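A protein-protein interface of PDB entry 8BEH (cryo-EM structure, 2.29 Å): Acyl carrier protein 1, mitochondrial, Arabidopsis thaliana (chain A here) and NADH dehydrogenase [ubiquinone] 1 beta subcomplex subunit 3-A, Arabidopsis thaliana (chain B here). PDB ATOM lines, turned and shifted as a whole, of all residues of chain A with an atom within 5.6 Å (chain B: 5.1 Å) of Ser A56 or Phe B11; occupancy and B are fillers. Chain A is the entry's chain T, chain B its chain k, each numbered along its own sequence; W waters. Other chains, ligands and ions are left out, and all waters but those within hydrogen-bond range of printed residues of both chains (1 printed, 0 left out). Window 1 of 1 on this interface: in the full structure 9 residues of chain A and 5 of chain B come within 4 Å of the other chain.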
ATOM      1  N   LEU A  51      -0.762   5.178  37.575  1.00  0.00           N
ATOM      2  CA  LEU A  51       0.519   5.109  38.266  1.00  0.00           C
ATOM      3  C   LEU A  51       1.474   4.143  37.580  1.00  0.00           C
ATOM      4  O   LEU A  51       2.689   4.352  37.612  1.00  0.00           O
ATOM      5  CB  LEU A  51       0.309   4.723  39.731  1.00  0.00           C
ATOM      6  CG  LEU A  51       0.463   5.862  40.750  1.00  0.00           C
ATOM      7  CD1 LEU A  51      -0.281   7.119  40.307  1.00  0.00           C
ATOM      8  CD2 LEU A  51      -0.003   5.428  42.124  1.00  0.00           C
ATOM      9  N   ASP A  52       0.953   3.085  36.951  1.00  0.00           N
ATOM     10  CA  ASP A  52       1.814   2.216  36.156  1.00  0.00           C
ATOM     11  C   ASP A  52       2.377   2.952  34.950  1.00  0.00           C
ATOM     12  O   ASP A  52       3.558   2.800  34.618  1.00  0.00           O
ATOM     13  CB  ASP A  52       1.054   0.965  35.714  1.00  0.00           C
ATOM     14  CG  ASP A  52       0.594   0.121  36.880  1.00  0.00           C
ATOM     15  OD1 ASP A  52       1.199   0.225  37.966  1.00  0.00           O
ATOM     16  OD2 ASP A  52      -0.378  -0.645  36.710  1.00  0.00           O
ATOM     17  N   VAL A  53       1.547   3.762  34.283  1.00  0.00           N
ATOM     18  CA  VAL A  53       2.035   4.541  33.147  1.00  0.00           C
ATOM     19  C   VAL A  53       3.155   5.477  33.589  1.00  0.00           C
ATOM     20  O   VAL A  53       4.216   5.547  32.958  1.00  0.00           O
ATOM     21  CB  VAL A  53       0.885   5.320  32.484  1.00  0.00           C
ATOM     22  CG1 VAL A  53       1.439   6.366  31.533  1.00  0.00           C
ATOM     23  CG2 VAL A  53      -0.050   4.376  31.744  1.00  0.00           C
ATOM     24  N   VAL A  54       2.943   6.191  34.696  1.00  0.00           N
ATOM     25  CA  VAL A  54       3.956   7.136  35.167  1.00  0.00           C
ATOM     26  C   VAL A  54       5.214   6.400  35.619  1.00  0.00           C
ATOM     27  O   VAL A  54       6.335   6.888  35.434  1.00  0.00           O
ATOM     28  CB  VAL A  54       3.388   8.033  36.282  1.00  0.00           C
ATOM     29  CG1 VAL A  54       4.371   9.130  36.625  1.00  0.00           C
ATOM     30  CG2 VAL A  54       2.061   8.641  35.852  1.00  0.00           C
ATOM     31  N   LYS A  55       5.051   5.217  36.212  1.00  0.00           N
ATOM     32  CA  LYS A  55       6.189   4.447  36.694  1.00  0.00           C
ATOM     33  C   LYS A  55       7.134   4.034  35.571  1.00  0.00           C
ATOM     34  O   LYS A  55       8.328   3.849  35.820  1.00  0.00           O
ATOM     35  CB  LYS A  55       5.691   3.206  37.432  1.00  0.00           C
ATOM     36  CG  LYS A  55       5.905   3.226  38.931  1.00  0.00           C
ATOM     37  CD  LYS A  55       4.834   2.403  39.633  1.00  0.00           C
ATOM     38  CE  LYS A  55       4.563   2.909  41.027  1.00  0.00           C
ATOM     39  NZ  LYS A  55       3.951   1.862  41.892  1.00  0.00           N
ATOM     40  N   SER A  56       6.634   3.903  34.343  1.00  0.00           N
ATOM     41  CA  SER A  56       7.460   3.457  33.231  1.00  0.00           C
ATOM     42  C   SER A  56       8.390   4.540  32.700  1.00  0.00           C
ATOM     43  O   SER A  56       9.217   4.243  31.833  1.00  0.00           O
ATOM     44  CB  SER A  56       6.582   2.954  32.083  1.00  0.00           C
ATOM     45  OG  SER A  56       5.425   2.308  32.562  1.00  0.00           O
ATOM     46  N   PHE A  57       8.271   5.774  33.174  1.00  0.00           N
ATOM     47  CA  PHE A  57       9.118   6.837  32.648  1.00  0.00           C
ATOM     48  C   PHE A  57      10.549   6.671  33.149  1.00  0.00           C
ATOM     49  O   PHE A  57      10.758   6.458  34.346  1.00  0.00           O
ATOM     50  CB  PHE A  57       8.582   8.207  33.030  1.00  0.00           C
ATOM     51  CG  PHE A  57       9.011   9.289  32.095  1.00  0.00           C
ATOM     52  CD1 PHE A  57       8.421   9.412  30.851  1.00  0.00           C
ATOM     53  CD2 PHE A  57      10.016  10.169  32.446  1.00  0.00           C
ATOM     54  CE1 PHE A  57       8.820  10.394  29.979  1.00  0.00           C
ATOM     55  CE2 PHE A  57      10.417  11.156  31.574  1.00  0.00           C
ATOM     56  CZ  PHE A  57       9.819  11.269  30.343  1.00  0.00           C
ATOM     57  N   PRO A  58      11.547   6.772  32.268  1.00  0.00           N
ATOM     58  CA  PRO A  58      12.927   6.452  32.686  1.00  0.00           C
ATOM     59  C   PRO A  58      13.496   7.383  33.747  1.00  0.00           C
ATOM     60  O   PRO A  58      14.127   6.905  34.698  1.00  0.00           O
ATOM     61  CB  PRO A  58      13.713   6.525  31.369  1.00  0.00           C
ATOM     62  CG  PRO A  58      12.838   7.240  30.407  1.00  0.00           C
ATOM     63  CD  PRO A  58      11.433   6.992  30.819  1.00  0.00           C
ATOM     64  N   GLU A  84       4.647  13.906  27.066  1.00  0.00           N
ATOM     65  CA  GLU A  84       4.799  12.496  26.713  1.00  0.00           C
ATOM     66  C   GLU A  84       3.980  11.591  27.629  1.00  0.00           C
ATOM     67  O   GLU A  84       3.337  10.644  27.162  1.00  0.00           O
ATOM     68  CB  GLU A  84       6.275  12.099  26.744  1.00  0.00           C
ATOM     69  CG  GLU A  84       7.097  12.695  25.614  1.00  0.00           C
ATOM     70  CD  GLU A  84       8.547  12.889  25.990  1.00  0.00           C
ATOM     71  OE1 GLU A  84       8.988  12.287  26.988  1.00  0.00           O
ATOM     72  OE2 GLU A  84       9.253  13.637  25.283  1.00  0.00           O
ATOM     73  N   ILE A  85       3.994  11.861  28.937  1.00  0.00           N
ATOM     74  CA  ILE A  85       3.248  11.028  29.878  1.00  0.00           C
ATOM     75  C   ILE A  85       1.747  11.149  29.632  1.00  0.00           C
ATOM     76  O   ILE A  85       1.004  10.163  29.727  1.00  0.00           O
ATOM     77  CB  ILE A  85       3.620  11.384  31.332  1.00  0.00           C
ATOM     78  CG1 ILE A  85       4.959  10.755  31.721  1.00  0.00           C
ATOM     79  CG2 ILE A  85       2.544  10.920  32.302  1.00  0.00           C
ATOM     80  CD1 ILE A  85       5.864  11.667  32.520  1.00  0.00           C
ATOM     81  N   ALA A  88       0.927   9.065  26.744  1.00  0.00           N
ATOM     82  CA  ALA A  88       0.929   7.656  27.129  1.00  0.00           C
ATOM     83  C   ALA A  88      -0.355   7.276  27.860  1.00  0.00           C
ATOM     84  O   ALA A  88      -0.895   6.187  27.647  1.00  0.00           O
ATOM     85  CB  ALA A  88       2.150   7.345  27.987  1.00  0.00           C
ATOM     86  N   GLY B   6      16.509   7.526  22.423  1.00  0.00           N
ATOM     87  CA  GLY B   6      16.171   8.696  23.258  1.00  0.00           C
ATOM     88  C   GLY B   6      15.208   8.405  24.381  1.00  0.00           C
ATOM     89  O   GLY B   6      14.498   7.420  24.299  1.00  0.00           O
ATOM     90  N   THR B   7      15.207   9.261  25.392  1.00  0.00           N
ATOM     91  CA  THR B   7      14.306   9.049  26.521  1.00  0.00           C
ATOM     92  C   THR B   7      12.856   8.893  26.065  1.00  0.00           C
ATOM     93  O   THR B   7      12.119   8.058  26.600  1.00  0.00           O
ATOM     94  CB  THR B   7      14.466  10.185  27.542  1.00  0.00           C
ATOM     95  OG1 THR B   7      13.897   9.795  28.795  1.00  0.00           O
ATOM     96  CG2 THR B   7      13.821  11.485  27.068  1.00  0.00           C
ATOM     97  N   THR B   8      12.445   9.645  25.043  1.00  0.00           N
ATOM     98  CA  THR B   8      11.064   9.580  24.570  1.00  0.00           C
ATOM     99  C   THR B   8      10.754   8.225  23.940  1.00  0.00           C
ATOM    100  O   THR B   8       9.762   7.569  24.295  1.00  0.00           O
ATOM    101  CB  THR B   8      10.818  10.712  23.572  1.00  0.00           C
ATOM    102  OG1 THR B   8      11.239  11.951  24.149  1.00  0.00           O
ATOM    103  CG2 THR B   8       9.350  10.803  23.201  1.00  0.00           C
ATOM    104  N   GLY B   9      11.600   7.789  23.005  1.00  0.00           N
ATOM    105  CA  GLY B   9      11.395   6.492  22.384  1.00  0.00           C
ATOM    106  C   GLY B   9      11.527   5.350  23.369  1.00  0.00           C
ATOM    107  O   GLY B   9      10.830   4.342  23.259  1.00  0.00           O
ATOM    108  N   GLU B  10      12.426   5.493  24.342  1.00  0.00           N
ATOM    109  CA  GLU B  10      12.588   4.477  25.374  1.00  0.00           C
ATOM    110  C   GLU B  10      11.335   4.354  26.230  1.00  0.00           C
ATOM    111  O   GLU B  10      10.894   3.243  26.545  1.00  0.00           O
ATOM    112  CB  GLU B  10      13.806   4.817  26.232  1.00  0.00           C
ATOM    113  CG  GLU B  10      13.802   4.211  27.621  1.00  0.00           C
ATOM    114  CD  GLU B  10      13.845   2.703  27.612  1.00  0.00           C
ATOM    115  OE1 GLU B  10      14.309   2.118  26.609  1.00  0.00           O
ATOM    116  OE2 GLU B  10      13.417   2.099  28.615  1.00  0.00           O
ATOM    117  N   PHE B  11      10.742   5.487  26.608  1.00  0.00           N
ATOM    118  CA  PHE B  11       9.496   5.464  27.362  1.00  0.00           C
ATOM    119  C   PHE B  11       8.380   4.808  26.557  1.00  0.00           C
ATOM    120  O   PHE B  11       7.633   3.965  27.076  1.00  0.00           O
ATOM    121  CB  PHE B  11       9.135   6.895  27.760  1.00  0.00           C
ATOM    122  CG  PHE B  11       7.777   7.045  28.364  1.00  0.00           C
ATOM    123  CD1 PHE B  11       7.399   6.289  29.456  1.00  0.00           C
ATOM    124  CD2 PHE B  11       6.882   7.965  27.849  1.00  0.00           C
ATOM    125  CE1 PHE B  11       6.149   6.438  30.013  1.00  0.00           C
ATOM    126  CE2 PHE B  11       5.627   8.120  28.408  1.00  0.00           C
ATOM    127  CZ  PHE B  11       5.266   7.355  29.491  1.00  0.00           C
ATOM    128  N   PHE B  12       8.267   5.163  25.278  1.00  0.00           N
ATOM    129  CA  PHE B  12       7.184   4.599  24.479  1.00  0.00           C
ATOM    130  C   PHE B  12       7.396   3.112  24.201  1.00  0.00           C
ATOM    131  O   PHE B  12       6.425   2.356  24.136  1.00  0.00           O
ATOM    132  CB  PHE B  12       7.021   5.393  23.189  1.00  0.00           C
ATOM    133  CG  PHE B  12       6.284   6.684  23.381  1.00  0.00           C
ATOM    134  CD1 PHE B  12       5.024   6.693  23.955  1.00  0.00           C
ATOM    135  CD2 PHE B  12       6.856   7.889  23.010  1.00  0.00           C
ATOM    136  CE1 PHE B  12       4.342   7.881  24.146  1.00  0.00           C
ATOM    137  CE2 PHE B  12       6.177   9.080  23.201  1.00  0.00           C
ATOM    138  CZ  PHE B  12       4.922   9.076  23.768  1.00  0.00           C
ATOM    139  N   ARG B  13       8.646   2.671  24.054  1.00  0.00           N
ATOM    140  CA  ARG B  13       8.914   1.244  23.915  1.00  0.00           C
ATOM    141  C   ARG B  13       8.620   0.496  25.210  1.00  0.00           C
ATOM    142  O   ARG B  13       8.104  -0.627  25.179  1.00  0.00           O
ATOM    143  CB  ARG B  13      10.361   1.014  23.489  1.00  0.00           C
ATOM    144  CG  ARG B  13      10.665  -0.433  23.188  1.00  0.00           C
ATOM    145  CD  ARG B  13      12.137  -0.643  22.891  1.00  0.00           C
ATOM    146  NE  ARG B  13      13.033  -0.574  24.046  1.00  0.00           N
ATOM    147  CZ  ARG B  13      12.819  -1.081  25.258  1.00  0.00           C
ATOM    148  NH1 ARG B  13      11.755  -1.818  25.536  1.00  0.00           N
ATOM    149  NH2 ARG B  13      13.724  -0.876  26.212  1.00  0.00           N
ATOM    150  N   ARG B  14       8.939   1.103  26.355  1.00  0.00           N
ATOM    151  CA  ARG B  14       8.609   0.485  27.633  1.00  0.00           C
ATOM    152  C   ARG B  14       7.107   0.298  27.784  1.00  0.00           C
ATOM    153  O   ARG B  14       6.651  -0.739  28.275  1.00  0.00           O
ATOM    154  CB  ARG B  14       9.159   1.329  28.779  1.00  0.00           C
ATOM    155  CG  ARG B  14      10.555   0.951  29.197  1.00  0.00           C
ATOM    156  CD  ARG B  14      10.864   1.426  30.595  1.00  0.00           C
ATOM    157  NE  ARG B  14      12.247   1.863  30.729  1.00  0.00           N
ATOM    158  CZ  ARG B  14      12.666   2.771  31.596  1.00  0.00           C
ATOM    159  NH1 ARG B  14      11.831   3.365  32.432  1.00  0.00           N
ATOM    160  NH2 ARG B  14      13.956   3.086  31.632  1.00  0.00           N
ATOM    161  N   ARG B  15       6.319   1.296  27.373  1.00  0.00           N
ATOM    162  CA  ARG B  15       4.870   1.160  27.471  1.00  0.00           C
ATOM    163  C   ARG B  15       4.316   0.091  26.538  1.00  0.00           C
ATOM    164  O   ARG B  15       3.234  -0.441  26.804  1.00  0.00           O
ATOM    165  CB  ARG B  15       4.184   2.498  27.179  1.00  0.00           C
ATOM    166  CG  ARG B  15       4.549   3.617  28.142  1.00  0.00           C
ATOM    167  CD  ARG B  15       4.069   3.349  29.553  1.00  0.00           C
ATOM    168  NE  ARG B  15       2.699   2.855  29.591  1.00  0.00           N
ATOM    169  CZ  ARG B  15       2.250   1.950  30.448  1.00  0.00           C
ATOM    170  NH1 ARG B  15       3.031   1.432  31.380  1.00  0.00           N
ATOM    171  NH2 ARG B  15       0.981   1.565  30.375  1.00  0.00           N
HETATM  172  O   HOH W   1       0.488   3.988  27.481  1.00  0.00           O
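Of the 11 printed residues of chain A, 7 touch a printed residue of chain B. Hydrophobic or aromatic side chains of chain A that line the printed part of chain B: Val A53, Phe A57, Pro A58 and Ala A88. Hydrophobic or aromatic side chains of chain B that line the printed part of chain A: Phe B11. Among the printed residues, 14 pairs touch across the chains. Among the printed residues, no Asp or Glu carboxylate lies within 4 Å of a Lys or Arg side-chain nitrogen of the other chain.
NH1 of Arg B14 sits close to N of Pro A58, 3.4 Å away. OG of Ser A56 sits at hydrogen-bond distance from NH1 of Arg B15 (2.8 Å). The side-chain hydroxyl (OG1) of Thr B8 lies within hydrogen-bond range of the side-chain carboxylate (OE2) of Glu A84, at 2.8 Å. The backbone carbonyl oxygen (O) of Ser A56 is in hydrogen-bond range of the guanidinium group (NH1) of Arg B14 (2.8 Å).
Of chain B, only Phe B11, Arg B14 and Arg B15 come within 4 Å of Ser A56. Phe B11 touches just these residues of chain A: Val A53 (3.6 Å), Ser A56 (3.6 Å), Phe A57 (3.5 Å), Pro A58 (3.8 Å), Glu A84 (3.6 Å) and Ala A88 (3.5 Å). Of the printed residues of chain B, Ala A88 touches Phe B11 (3.5 Å). Of the printed residues of chain B, Glu A84 touches Thr B8 and Phe B11. Gly B9 touches none of the printed residues of chain A. The nearest printed residue of chain B that does not touch Ser A56 is Glu B10 (5.6 Å).
OE2 of Glu B10 is in salt-bridge range of NE of Arg B14, 2.4 Å away. The backbone carbonyl oxygen of Asp A52 sits at hydrogen-bond distance from the side-chain hydroxyl of Ser A56 (2.8 Å). The side-chain hydroxyl (OG) of Ser A56 sits at hydrogen-bond distance from the backbone carbonyl oxygen (O) of Val A53, at 3.5 Å.
Among the printed residues, merely in contact across the chains: Asp A52 with Arg B15 (3.6 Å), Val A53 with Phe B11 (3.6 Å), Val A53 with Arg B15 (3.3 Å), Ser A56 with Phe B11 (3.6 Å), Phe A57 with Phe B11 (3.5 Å), Phe A57 with Arg B14 (3.6 Å), Pro A58 with Thr B7 (3.2 Å), Pro A58 with Phe B11 (3.8 Å), Glu A84 with Phe B11 (3.6 Å) and Ala A88 with Phe B11 (3.5 Å).
Water W1 bridges O of Ala A88 (2.6 Å) and NE of Arg B15 (3.3 Å).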
